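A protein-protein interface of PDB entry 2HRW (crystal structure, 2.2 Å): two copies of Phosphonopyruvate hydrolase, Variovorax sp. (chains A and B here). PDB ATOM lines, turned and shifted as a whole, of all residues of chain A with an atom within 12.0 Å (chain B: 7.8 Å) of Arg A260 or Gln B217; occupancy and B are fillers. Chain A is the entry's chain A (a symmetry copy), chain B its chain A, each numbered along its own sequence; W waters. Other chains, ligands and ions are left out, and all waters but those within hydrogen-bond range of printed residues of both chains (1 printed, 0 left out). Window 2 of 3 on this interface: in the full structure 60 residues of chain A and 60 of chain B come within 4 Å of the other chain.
Printed residues of chain B within 4 Å of Gly A257: Glu B220. Of chain B, only Pro B216 (3.2 Å), Gln B217 (3.1 Å) and Thr B219 (3.2 Å) come within 4 Å of Arg A260. Ala A264 touches none of the printed residues of chain B. Of the printed residues of chain B, Leu A266 touches His B237. No residue of chain A comes within 4 Å of Lys B190. No residue of chain A comes within 4 Å of Thr B191. No residue of chain A comes within 4 Å of Pro B192. No residue of chain A comes within 4 Å of Ala B214. Of the printed residues of chain A, Gln B217 touches Arg A260. No residue of chain A comes within 4 Å of Leu B218. Thr B219 touches one residue of chain A. Printed residues of chain A within 4 Å of Tyr B234: Gly A258 (3.7 Å) and Ile A259 (3.7 Å). The nearest residue of chain A that does not touch Gln B217 is Ile A259 (5.6 Å). The nearest printed residue of chain B that does not touch Arg A254 is Tyr B234 (5.2 Å).
Water W1 lies within hydrogen-bond range of O of Leu B218 (2.7 Å), O of Pro B216 (3.2 Å) and N of Ile A259 (3.4 Å).
Tyr B234 touches Gly A258 (OH to CA, 3.7 Å). Pro B216 touches Ile A259. CE1 of Tyr B234 touches CG1 of Ile A259, 3.7 Å away. Arg A260 touches Pro B216 (CG to O, 3.2 Å). Thr B219 touches Arg A260 (CG2 to NH2, 3.2 Å). Pro B216 touches Asp A263 (CB to CG, 3.98 Å). Leu A266 touches His B237.
The side-chain carboxylate of Glu B220 is in salt-bridge range of the guanidinium group of Arg A254 (3.2 Å). The backbone NH (N) of Glu B220 lies close to the backbone carbonyl oxygen (O) of Gly A257 (3.3 Å). O of Gln B217 is in hydrogen-bond range of NH1 of Arg A260, at 3.1 Å.
OH of Tyr B234 sits at hydrogen-bond distance from OE1 of Glu B220 (2.8 Å). The backbone NH of Gly A258 is in hydrogen-bond range of the backbone carbonyl oxygen of Ile A253 (2.9 Å). The guanidinium group (NE) of Arg A260 is in salt-bridge range of the side-chain carboxylate (OE1) of Glu A261 (3.5 Å). The side-chain hydroxyl of Thr B219 is in hydrogen-bond range of the backbone NH of Asp B222 (3.1 Å). The side-chain amino group (NZ) of Lys B190 sits close to the side-chain amide nitrogen (NE2) of Gln B217. N of Ala B221 sits close to OG1 of Thr B219 (3.2 Å).
Among the printed residues, Asp or Glu carboxylates within 4 Å of a Lys or Arg side-chain nitrogen of the other chain: Arg A254 with Glu B220 (3.2 Å).
No position is printed for both chains. Of the 10 pairs that touch across the chains among the printed residues, none has its exchanged pair printed and touching as well.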
ATOM      1  N   GLU A 248      28.165   8.625  -1.544  1.00  0.00           N
ATOM      2  CA  GLU A 248      27.917   7.490  -0.649  1.00  0.00           C
ATOM      3  C   GLU A 248      26.550   6.841  -0.840  1.00  0.00           C
ATOM      4  O   GLU A 248      26.421   5.621  -0.717  1.00  0.00           O
ATOM      5  CB  GLU A 248      28.029   7.911   0.818  1.00  0.00           C
ATOM      6  CG  GLU A 248      27.637   6.809   1.816  1.00  0.00           C
ATOM      7  CD  GLU A 248      26.773   7.316   2.993  1.00  0.00           C
ATOM      8  OE1 GLU A 248      25.597   6.859   3.125  1.00  0.00           O
ATOM      9  OE2 GLU A 248      27.271   8.167   3.786  1.00  0.00           O
ATOM     10  N   VAL A 249      25.532   7.663  -1.096  1.00  0.00           N
ATOM     11  CA  VAL A 249      24.175   7.175  -1.285  1.00  0.00           C
ATOM     12  C   VAL A 249      24.014   6.477  -2.626  1.00  0.00           C
ATOM     13  O   VAL A 249      23.199   5.582  -2.753  1.00  0.00           O
ATOM     14  CB  VAL A 249      23.175   8.331  -1.172  1.00  0.00           C
ATOM     15  CG1 VAL A 249      21.810   7.896  -1.618  1.00  0.00           C
ATOM     16  CG2 VAL A 249      23.098   8.781   0.270  1.00  0.00           C
ATOM     17  N   PHE A 250      24.788   6.893  -3.625  1.00  0.00           N
ATOM     18  CA  PHE A 250      24.730   6.254  -4.946  1.00  0.00           C
ATOM     19  C   PHE A 250      25.460   4.917  -4.834  1.00  0.00           C
ATOM     20  O   PHE A 250      25.133   3.952  -5.532  1.00  0.00           O
ATOM     21  CB  PHE A 250      25.439   7.083  -6.035  1.00  0.00           C
ATOM     22  CG  PHE A 250      24.645   8.271  -6.555  1.00  0.00           C
ATOM     23  CD1 PHE A 250      23.332   8.505  -6.149  1.00  0.00           C
ATOM     24  CD2 PHE A 250      25.228   9.153  -7.479  1.00  0.00           C
ATOM     25  CE1 PHE A 250      22.612   9.596  -6.651  1.00  0.00           C
ATOM     26  CE2 PHE A 250      24.493  10.265  -7.995  1.00  0.00           C
ATOM     27  CZ  PHE A 250      23.192  10.478  -7.579  1.00  0.00           C
ATOM     28  N   ALA A 251      26.449   4.851  -3.953  1.00  0.00           N
ATOM     29  CA  ALA A 251      27.204   3.617  -3.795  1.00  0.00           C
ATOM     30  C   ALA A 251      26.345   2.593  -3.053  1.00  0.00           C
ATOM     31  O   ALA A 251      26.295   1.411  -3.437  1.00  0.00           O
ATOM     32  CB  ALA A 251      28.493   3.886  -3.052  1.00  0.00           C
ATOM     33  N   ARG A 252      25.658   3.047  -2.001  1.00  0.00           N
ATOM     34  CA  ARG A 252      24.791   2.147  -1.255  1.00  0.00           C
ATOM     35  C   ARG A 252      23.657   1.598  -2.140  1.00  0.00           C
ATOM     36  O   ARG A 252      23.394   0.407  -2.112  1.00  0.00           O
ATOM     37  CB  ARG A 252      24.188   2.837  -0.020  1.00  0.00           C
ATOM     38  CG  ARG A 252      25.192   3.253   1.046  1.00  0.00           C
ATOM     39  CD  ARG A 252      24.477   3.830   2.262  1.00  0.00           C
ATOM     40  NE  ARG A 252      23.601   2.834   2.884  1.00  0.00           N
ATOM     41  CZ  ARG A 252      22.800   3.056   3.929  1.00  0.00           C
ATOM     42  NH1 ARG A 252      22.738   4.257   4.495  1.00  0.00           N
ATOM     43  NH2 ARG A 252      22.064   2.061   4.419  1.00  0.00           N
ATOM     44  N   ILE A 253      22.991   2.454  -2.916  1.00  0.00           N
ATOM     45  CA  ILE A 253      21.892   2.014  -3.779  1.00  0.00           C
ATOM     46  C   ILE A 253      22.312   0.920  -4.766  1.00  0.00           C
ATOM     47  O   ILE A 253      21.591  -0.063  -4.946  1.00  0.00           O
ATOM     48  CB  ILE A 253      21.284   3.197  -4.577  1.00  0.00           C
ATOM     49  CG1 ILE A 253      20.607   4.176  -3.604  1.00  0.00           C
ATOM     50  CG2 ILE A 253      20.287   2.665  -5.614  1.00  0.00           C
ATOM     51  CD1 ILE A 253      20.042   5.443  -4.218  1.00  0.00           C
ATOM     52  N   ARG A 254      23.480   1.089  -5.385  1.00  0.00           N
ATOM     53  CA  ARG A 254      24.028   0.128  -6.349  1.00  0.00           C
ATOM     54  C   ARG A 254      24.674  -1.100  -5.681  1.00  0.00           C
ATOM     55  O   ARG A 254      24.960  -2.105  -6.339  1.00  0.00           O
ATOM     56  CB  ARG A 254      25.062   0.821  -7.241  1.00  0.00           C
ATOM     57  CG  ARG A 254      24.472   1.785  -8.248  1.00  0.00           C
ATOM     58  CD  ARG A 254      24.576   1.236  -9.650  1.00  0.00           C
ATOM     59  NE  ARG A 254      23.935  -0.061  -9.818  1.00  0.00           N
ATOM     60  CZ  ARG A 254      22.620  -0.259  -9.743  1.00  0.00           C
ATOM     61  NH1 ARG A 254      22.110  -1.479  -9.912  1.00  0.00           N
ATOM     62  NH2 ARG A 254      21.808   0.761  -9.494  1.00  0.00           N
ATOM     63  N   ARG A 255      24.932  -1.008  -4.384  1.00  0.00           N
ATOM     64  CA  ARG A 255      25.503  -2.134  -3.672  1.00  0.00           C
ATOM     65  C   ARG A 255      24.325  -2.913  -3.085  1.00  0.00           C
ATOM     66  O   ARG A 255      24.344  -4.138  -3.037  1.00  0.00           O
ATOM     67  CB  ARG A 255      26.416  -1.624  -2.569  1.00  0.00           C
ATOM     68  CG  ARG A 255      27.615  -2.505  -2.270  1.00  0.00           C
ATOM     69  CD  ARG A 255      28.606  -1.723  -1.425  1.00  0.00           C
ATOM     70  NE  ARG A 255      27.919  -0.992  -0.366  1.00  0.00           N
ATOM     71  CZ  ARG A 255      28.125   0.289  -0.076  1.00  0.00           C
ATOM     72  NH1 ARG A 255      29.003   1.002  -0.757  1.00  0.00           N
ATOM     73  NH2 ARG A 255      27.436   0.864   0.896  1.00  0.00           N
ATOM     74  N   ASP A 256      23.288  -2.200  -2.649  1.00  0.00           N
ATOM     75  CA  ASP A 256      22.089  -2.834  -2.083  1.00  0.00           C
ATOM     76  C   ASP A 256      21.095  -3.230  -3.195  1.00  0.00           C
ATOM     77  O   ASP A 256      20.170  -4.028  -2.970  1.00  0.00           O
ATOM     78  CB  ASP A 256      21.378  -1.879  -1.099  1.00  0.00           C
ATOM     79  CG  ASP A 256      22.280  -1.420   0.041  1.00  0.00           C
ATOM     80  OD1 ASP A 256      21.869  -0.492   0.790  1.00  0.00           O
ATOM     81  OD2 ASP A 256      23.391  -1.985   0.179  1.00  0.00           O
ATOM     82  N   GLY A 257      21.286  -2.676  -4.390  1.00  0.00           N
ATOM     83  CA  GLY A 257      20.375  -2.977  -5.477  1.00  0.00           C
ATOM     84  C   GLY A 257      18.987  -2.447  -5.156  1.00  0.00           C
ATOM     85  O   GLY A 257      17.988  -3.119  -5.367  1.00  0.00           O
ATOM     86  N   GLY A 258      18.923  -1.231  -4.631  1.00  0.00           N
ATOM     87  CA  GLY A 258      17.645  -0.641  -4.289  1.00  0.00           C
ATOM     88  C   GLY A 258      17.833   0.428  -3.231  1.00  0.00           C
ATOM     89  O   GLY A 258      18.967   0.753  -2.861  1.00  0.00           O
ATOM     90  N   ILE A 259      16.727   0.982  -2.745  1.00  0.00           N
ATOM     91  CA  ILE A 259      16.786   2.029  -1.727  1.00  0.00           C
ATOM     92  C   ILE A 259      15.936   1.653  -0.522  1.00  0.00           C
ATOM     93  O   ILE A 259      15.229   2.482   0.045  1.00  0.00           O
ATOM     94  CB  ILE A 259      16.308   3.374  -2.307  1.00  0.00           C
ATOM     95  CG1 ILE A 259      15.011   3.200  -3.100  1.00  0.00           C
ATOM     96  CG2 ILE A 259      17.342   3.906  -3.259  1.00  0.00           C
ATOM     97  CD1 ILE A 259      13.794   3.065  -2.288  1.00  0.00           C
ATOM     98  N   ARG A 260      16.005   0.388  -0.130  1.00  0.00           N
ATOM     99  CA  ARG A 260      15.221  -0.068   0.996  1.00  0.00           C
ATOM    100  C   ARG A 260      15.950   0.243   2.279  1.00  0.00           C
ATOM    101  O   ARG A 260      15.315   0.560   3.266  1.00  0.00           O
ATOM    102  CB  ARG A 260      14.959  -1.574   0.904  1.00  0.00           C
ATOM    103  CG  ARG A 260      13.776  -2.018   1.743  1.00  0.00           C
ATOM    104  CD  ARG A 260      14.140  -3.178   2.650  1.00  0.00           C
ATOM    105  NE  ARG A 260      14.677  -4.326   1.919  1.00  0.00           N
ATOM    106  CZ  ARG A 260      13.954  -5.174   1.188  1.00  0.00           C
ATOM    107  NH1 ARG A 260      12.635  -5.029   1.070  1.00  0.00           N
ATOM    108  NH2 ARG A 260      14.559  -6.179   0.570  1.00  0.00           N
ATOM    109  N   GLU A 261      17.278   0.146   2.256  1.00  0.00           N
ATOM    110  CA  GLU A 261      18.116   0.408   3.429  1.00  0.00           C
ATOM    111  C   GLU A 261      18.427   1.894   3.573  1.00  0.00           C
ATOM    112  O   GLU A 261      18.481   2.433   4.680  1.00  0.00           O
ATOM    113  CB  GLU A 261      19.463  -0.322   3.315  1.00  0.00           C
ATOM    114  CG  GLU A 261      19.500  -1.755   3.800  1.00  0.00           C
ATOM    115  CD  GLU A 261      18.520  -2.651   3.053  1.00  0.00           C
ATOM    116  OE1 GLU A 261      17.304  -2.592   3.356  1.00  0.00           O
ATOM    117  OE2 GLU A 261      18.972  -3.409   2.157  1.00  0.00           O
ATOM    118  N   VAL A 262      18.615   2.547   2.434  1.00  0.00           N
ATOM    119  CA  VAL A 262      19.004   3.940   2.399  1.00  0.00           C
ATOM    120  C   VAL A 262      17.898   4.982   2.583  1.00  0.00           C
ATOM    121  O   VAL A 262      18.165   6.089   3.083  1.00  0.00           O
ATOM    122  CB  VAL A 262      19.769   4.194   1.091  1.00  0.00           C
ATOM    123  CG1 VAL A 262      18.791   4.359  -0.028  1.00  0.00           C
ATOM    124  CG2 VAL A 262      20.694   5.369   1.229  1.00  0.00           C
ATOM    125  N   ASP A 263      16.664   4.637   2.216  1.00  0.00           N
ATOM    126  CA  ASP A 263      15.544   5.589   2.330  1.00  0.00           C
ATOM    127  C   ASP A 263      15.332   6.167   3.734  1.00  0.00           C
ATOM    128  O   ASP A 263      15.039   7.354   3.886  1.00  0.00           O
ATOM    129  CB  ASP A 263      14.241   4.934   1.852  1.00  0.00           C
ATOM    130  CG  ASP A 263      13.021   5.790   2.137  1.00  0.00           C
ATOM    131  OD1 ASP A 263      12.532   5.785   3.296  1.00  0.00           O
ATOM    132  OD2 ASP A 263      12.553   6.488   1.206  1.00  0.00           O
ATOM    133  N   ALA A 264      15.479   5.306   4.744  1.00  0.00           N
ATOM    134  CA  ALA A 264      15.306   5.666   6.143  1.00  0.00           C
ATOM    135  C   ALA A 264      16.228   6.807   6.609  1.00  0.00           C
ATOM    136  O   ALA A 264      15.803   7.692   7.345  1.00  0.00           O
ATOM    137  CB  ALA A 264      15.542   4.425   6.998  1.00  0.00           C
ATOM    138  N   ALA A 265      17.482   6.758   6.169  1.00  0.00           N
ATOM    139  CA  ALA A 265      18.509   7.745   6.499  1.00  0.00           C
ATOM    140  C   ALA A 265      18.408   9.063   5.711  1.00  0.00           C
ATOM    141  O   ALA A 265      19.276   9.919   5.827  1.00  0.00           O
ATOM    142  CB  ALA A 265      19.889   7.134   6.265  1.00  0.00           C
ATOM    143  N   LEU A 266      17.362   9.242   4.923  1.00  0.00           N
ATOM    144  CA  LEU A 266      17.253  10.457   4.127  1.00  0.00           C
ATOM    145  C   LEU A 266      16.214  11.448   4.591  1.00  0.00           C
ATOM    146  O   LEU A 266      15.286  11.100   5.303  1.00  0.00           O
ATOM    147  CB  LEU A 266      16.903  10.096   2.682  1.00  0.00           C
ATOM    148  CG  LEU A 266      17.908   9.276   1.876  1.00  0.00           C
ATOM    149  CD1 LEU A 266      17.342   8.973   0.484  1.00  0.00           C
ATOM    150  CD2 LEU A 266      19.235  10.038   1.824  1.00  0.00           C
ATOM    151  N   GLN B 189      -0.718   5.232  -2.884  1.00  0.00           N
ATOM    152  CA  GLN B 189      -0.647   4.249  -1.800  1.00  0.00           C
ATOM    153  C   GLN B 189       0.722   4.135  -1.170  1.00  0.00           C
ATOM    154  O   GLN B 189       1.743   4.229  -1.861  1.00  0.00           O
ATOM    155  CB  GLN B 189      -1.037   2.861  -2.322  1.00  0.00           C
ATOM    156  CG  GLN B 189      -2.474   2.487  -2.064  1.00  0.00           C
ATOM    157  CD  GLN B 189      -3.455   3.310  -2.862  1.00  0.00           C
ATOM    158  OE1 GLN B 189      -3.218   4.485  -3.140  1.00  0.00           O
ATOM    159  NE2 GLN B 189      -4.577   2.700  -3.223  1.00  0.00           N
ATOM    160  N   LYS B 190       0.761   3.913   0.138  1.00  0.00           N
ATOM    161  CA  LYS B 190       2.063   3.760   0.774  1.00  0.00           C
ATOM    162  C   LYS B 190       2.554   2.325   0.582  1.00  0.00           C
ATOM    163  O   LYS B 190       3.715   2.019   0.869  1.00  0.00           O
ATOM    164  CB  LYS B 190       2.014   4.118   2.261  1.00  0.00           C
ATOM    165  CG  LYS B 190       3.117   5.095   2.681  1.00  0.00           C
ATOM    166  CD  LYS B 190       4.511   4.634   2.231  1.00  0.00           C
ATOM    167  CE  LYS B 190       4.982   3.371   2.971  1.00  0.00           C
ATOM    168  NZ  LYS B 190       6.281   2.817   2.459  1.00  0.00           N
ATOM    169  N   THR B 191       1.661   1.455   0.086  1.00  0.00           N
ATOM    170  CA  THR B 191       1.989   0.051  -0.205  1.00  0.00           C
ATOM    171  C   THR B 191       1.961  -0.152  -1.718  1.00  0.00           C
ATOM    172  O   THR B 191       1.093   0.395  -2.411  1.00  0.00           O
ATOM    173  CB  THR B 191       0.969  -0.904   0.372  1.00  0.00           C
ATOM    174  OG1 THR B 191      -0.193  -0.912  -0.463  1.00  0.00           O
ATOM    175  CG2 THR B 191       0.577  -0.467   1.748  1.00  0.00           C
ATOM    176  N   PRO B 192       2.899  -0.950  -2.252  1.00  0.00           N
ATOM    177  CA  PRO B 192       2.945  -1.194  -3.686  1.00  0.00           C
ATOM    178  C   PRO B 192       1.895  -2.188  -4.155  1.00  0.00           C
ATOM    179  O   PRO B 192       2.172  -2.980  -5.043  1.00  0.00           O
ATOM    180  CB  PRO B 192       4.356  -1.718  -3.892  1.00  0.00           C
ATOM    181  CG  PRO B 192       4.559  -2.524  -2.683  1.00  0.00           C
ATOM    182  CD  PRO B 192       4.021  -1.632  -1.588  1.00  0.00           C
ATOM    183  N   ASP B 193       0.701  -2.151  -3.555  1.00  0.00           N
ATOM    184  CA  ASP B 193      -0.384  -3.055  -3.939  1.00  0.00           C
ATOM    185  C   ASP B 193      -1.026  -2.564  -5.222  1.00  0.00           C
ATOM    186  O   ASP B 193      -1.263  -3.332  -6.154  1.00  0.00           O
ATOM    187  CB  ASP B 193      -1.462  -3.122  -2.851  1.00  0.00           C
ATOM    188  CG  ASP B 193      -1.031  -3.929  -1.634  1.00  0.00           C
ATOM    189  OD1 ASP B 193      -1.879  -4.156  -0.738  1.00  0.00           O
ATOM    190  OD2 ASP B 193       0.151  -4.337  -1.567  1.00  0.00           O
ATOM    191  N   PRO B 212       9.078   4.028  -7.868  1.00  0.00           N
ATOM    192  CA  PRO B 212       8.734   3.463  -6.550  1.00  0.00           C
ATOM    193  C   PRO B 212       9.132   4.257  -5.321  1.00  0.00           C
ATOM    194  O   PRO B 212       9.414   3.688  -4.264  1.00  0.00           O
ATOM    195  CB  PRO B 212       9.429   2.112  -6.577  1.00  0.00           C
ATOM    196  CG  PRO B 212      10.737   2.476  -7.256  1.00  0.00           C
ATOM    197  CD  PRO B 212      10.242   3.316  -8.437  1.00  0.00           C
ATOM    198  N   THR B 213       9.140   5.573  -5.464  1.00  0.00           N
ATOM    199  CA  THR B 213       9.521   6.479  -4.386  1.00  0.00           C
ATOM    200  C   THR B 213       8.721   6.318  -3.086  1.00  0.00           C
ATOM    201  O   THR B 213       9.295   6.365  -1.993  1.00  0.00           O
ATOM    202  CB  THR B 213       9.430   7.957  -4.886  1.00  0.00           C
ATOM    203  OG1 THR B 213      10.406   8.169  -5.917  1.00  0.00           O
ATOM    204  CG2 THR B 213       9.689   8.927  -3.750  1.00  0.00           C
ATOM    205  N   ALA B 214       7.409   6.107  -3.200  1.00  0.00           N
ATOM    206  CA  ALA B 214       6.541   5.967  -2.016  1.00  0.00           C
ATOM    207  C   ALA B 214       6.548   4.582  -1.373  1.00  0.00           C
ATOM    208  O   ALA B 214       6.172   4.431  -0.210  1.00  0.00           O
ATOM    209  CB  ALA B 214       5.098   6.352  -2.384  1.00  0.00           C
ATOM    210  N   TYR B 215       6.940   3.568  -2.141  1.00  0.00           N
ATOM    211  CA  TYR B 215       6.991   2.206  -1.619  1.00  0.00           C
ATOM    212  C   TYR B 215       8.416   1.685  -1.755  1.00  0.00           C
ATOM    213  O   TYR B 215       8.740   0.880  -2.626  1.00  0.00           O
ATOM    214  CB  TYR B 215       5.981   1.306  -2.349  1.00  0.00           C
ATOM    215  CG  TYR B 215       5.333   1.963  -3.529  1.00  0.00           C
ATOM    216  CD1 TYR B 215       6.048   2.143  -4.710  1.00  0.00           C
ATOM    217  CD2 TYR B 215       4.027   2.467  -3.454  1.00  0.00           C
ATOM    218  CE1 TYR B 215       5.502   2.812  -5.798  1.00  0.00           C
ATOM    219  CE2 TYR B 215       3.456   3.149  -4.541  1.00  0.00           C
ATOM    220  CZ  TYR B 215       4.214   3.322  -5.720  1.00  0.00           C
ATOM    221  OH  TYR B 215       3.734   4.035  -6.822  1.00  0.00           O
ATOM    222  N   PRO B 216       9.297   2.162  -0.871  1.00  0.00           N
ATOM    223  CA  PRO B 216      10.707   1.785  -0.843  1.00  0.00           C
ATOM    224  C   PRO B 216      10.977   0.344  -0.415  1.00  0.00           C
ATOM    225  O   PRO B 216      12.128  -0.038  -0.208  1.00  0.00           O
ATOM    226  CB  PRO B 216      11.314   2.809   0.122  1.00  0.00           C
ATOM    227  CG  PRO B 216      10.197   3.075   1.065  1.00  0.00           C
ATOM    228  CD  PRO B 216       9.013   3.192   0.145  1.00  0.00           C
ATOM    229  N   GLN B 217       9.930  -0.458  -0.270  1.00  0.00           N
ATOM    230  CA  GLN B 217      10.134  -1.842   0.143  1.00  0.00           C
ATOM    231  C   GLN B 217      10.287  -2.702  -1.101  1.00  0.00           C
ATOM    232  O   GLN B 217      10.745  -3.850  -1.045  1.00  0.00           O
ATOM    233  CB  GLN B 217       8.963  -2.316   1.003  1.00  0.00           C
ATOM    234  CG  GLN B 217       7.588  -2.064   0.409  1.00  0.00           C
ATOM    235  CD  GLN B 217       6.914  -0.789   0.920  1.00  0.00           C
ATOM    236  OE1 GLN B 217       5.740  -0.560   0.640  1.00  0.00           O
ATOM    237  NE2 GLN B 217       7.645   0.038   1.670  1.00  0.00           N
ATOM    238  N   LEU B 218       9.921  -2.097  -2.227  1.00  0.00           N
ATOM    239  CA  LEU B 218       9.984  -2.732  -3.539  1.00  0.00           C
ATOM    240  C   LEU B 218      11.403  -2.562  -4.108  1.00  0.00           C
ATOM    241  O   LEU B 218      11.739  -1.496  -4.629  1.00  0.00           O
ATOM    242  CB  LEU B 218       8.950  -2.072  -4.475  1.00  0.00           C
ATOM    243  CG  LEU B 218       8.282  -2.934  -5.551  1.00  0.00           C
ATOM    244  CD1 LEU B 218       7.583  -2.059  -6.593  1.00  0.00           C
ATOM    245  CD2 LEU B 218       9.333  -3.767  -6.231  1.00  0.00           C
ATOM    246  N   THR B 219      12.213  -3.618  -4.014  1.00  0.00           N
ATOM    247  CA  THR B 219      13.597  -3.595  -4.489  1.00  0.00           C
ATOM    248  C   THR B 219      13.730  -3.791  -6.009  1.00  0.00           C
ATOM    249  O   THR B 219      12.741  -4.073  -6.699  1.00  0.00           O
ATOM    250  CB  THR B 219      14.464  -4.691  -3.773  1.00  0.00           C
ATOM    251  OG1 THR B 219      14.137  -5.989  -4.288  1.00  0.00           O
ATOM    252  CG2 THR B 219      14.196  -4.681  -2.268  1.00  0.00           C
ATOM    253  N   GLU B 220      14.947  -3.627  -6.526  1.00  0.00           N
ATOM    254  CA  GLU B 220      15.178  -3.810  -7.952  1.00  0.00           C
ATOM    255  C   GLU B 220      14.929  -5.284  -8.271  1.00  0.00           C
ATOM    256  O   GLU B 220      14.509  -5.613  -9.372  1.00  0.00           O
ATOM    257  CB  GLU B 220      16.610  -3.396  -8.340  1.00  0.00           C
ATOM    258  CG  GLU B 220      16.887  -1.877  -8.242  1.00  0.00           C
ATOM    259  CD  GLU B 220      18.265  -1.443  -8.770  1.00  0.00           C
ATOM    260  OE1 GLU B 220      18.567  -0.220  -8.740  1.00  0.00           O
ATOM    261  OE2 GLU B 220      19.052  -2.310  -9.216  1.00  0.00           O
ATOM    262  N   ALA B 221      15.173  -6.163  -7.295  1.00  0.00           N
ATOM    263  CA  ALA B 221      14.938  -7.598  -7.487  1.00  0.00           C
ATOM    264  C   ALA B 221      13.429  -7.832  -7.608  1.00  0.00           C
ATOM    265  O   ALA B 221      12.970  -8.630  -8.436  1.00  0.00           O
ATOM    266  CB  ALA B 221      15.497  -8.415  -6.307  1.00  0.00           C
ATOM    267  N   ASP B 222      12.655  -7.151  -6.771  1.00  0.00           N
ATOM    268  CA  ASP B 222      11.219  -7.303  -6.848  1.00  0.00           C
ATOM    269  C   ASP B 222      10.715  -6.753  -8.185  1.00  0.00           C
ATOM    270  O   ASP B 222       9.819  -7.322  -8.794  1.00  0.00           O
ATOM    271  CB  ASP B 222      10.529  -6.573  -5.700  1.00  0.00           C
ATOM    272  CG  ASP B 222      10.547  -7.353  -4.407  1.00  0.00           C
ATOM    273  OD1 ASP B 222      10.255  -8.575  -4.439  1.00  0.00           O
ATOM    274  OD2 ASP B 222      10.838  -6.730  -3.354  1.00  0.00           O
ATOM    275  N   TYR B 234      14.643   6.378  -9.806  1.00  0.00           N
ATOM    276  CA  TYR B 234      14.774   6.890  -8.452  1.00  0.00           C
ATOM    277  C   TYR B 234      14.500   8.385  -8.534  1.00  0.00           C
ATOM    278  O   TYR B 234      15.359   9.171  -8.919  1.00  0.00           O
ATOM    279  CB  TYR B 234      16.168   6.576  -7.950  1.00  0.00           C
ATOM    280  CG  TYR B 234      16.325   5.065  -7.803  1.00  0.00           C
ATOM    281  CD1 TYR B 234      15.574   4.381  -6.863  1.00  0.00           C
ATOM    282  CD2 TYR B 234      17.141   4.320  -8.657  1.00  0.00           C
ATOM    283  CE1 TYR B 234      15.622   2.995  -6.762  1.00  0.00           C
ATOM    284  CE2 TYR B 234      17.189   2.907  -8.563  1.00  0.00           C
ATOM    285  CZ  TYR B 234      16.420   2.272  -7.602  1.00  0.00           C
ATOM    286  OH  TYR B 234      16.414   0.916  -7.441  1.00  0.00           O
ATOM    287  N   HIS B 237      16.044  11.114  -4.625  1.00  0.00           N
ATOM    288  CA  HIS B 237      17.026  10.794  -3.629  1.00  0.00           C
ATOM    289  C   HIS B 237      18.260  11.685  -3.718  1.00  0.00           C
ATOM    290  O   HIS B 237      18.950  11.882  -2.712  1.00  0.00           O
ATOM    291  CB  HIS B 237      17.345   9.296  -3.733  1.00  0.00           C
ATOM    292  CG  HIS B 237      16.112   8.440  -3.698  1.00  0.00           C
ATOM    293  ND1 HIS B 237      15.311   8.248  -4.806  1.00  0.00           N
ATOM    294  CD2 HIS B 237      15.471   7.841  -2.664  1.00  0.00           C
ATOM    295  CE1 HIS B 237      14.229   7.573  -4.450  1.00  0.00           C
ATOM    296  NE2 HIS B 237      14.303   7.316  -3.155  1.00  0.00           N
HETATM  297  O   HOH W   1      13.631  -0.479  -3.040  1.00  0.00           O
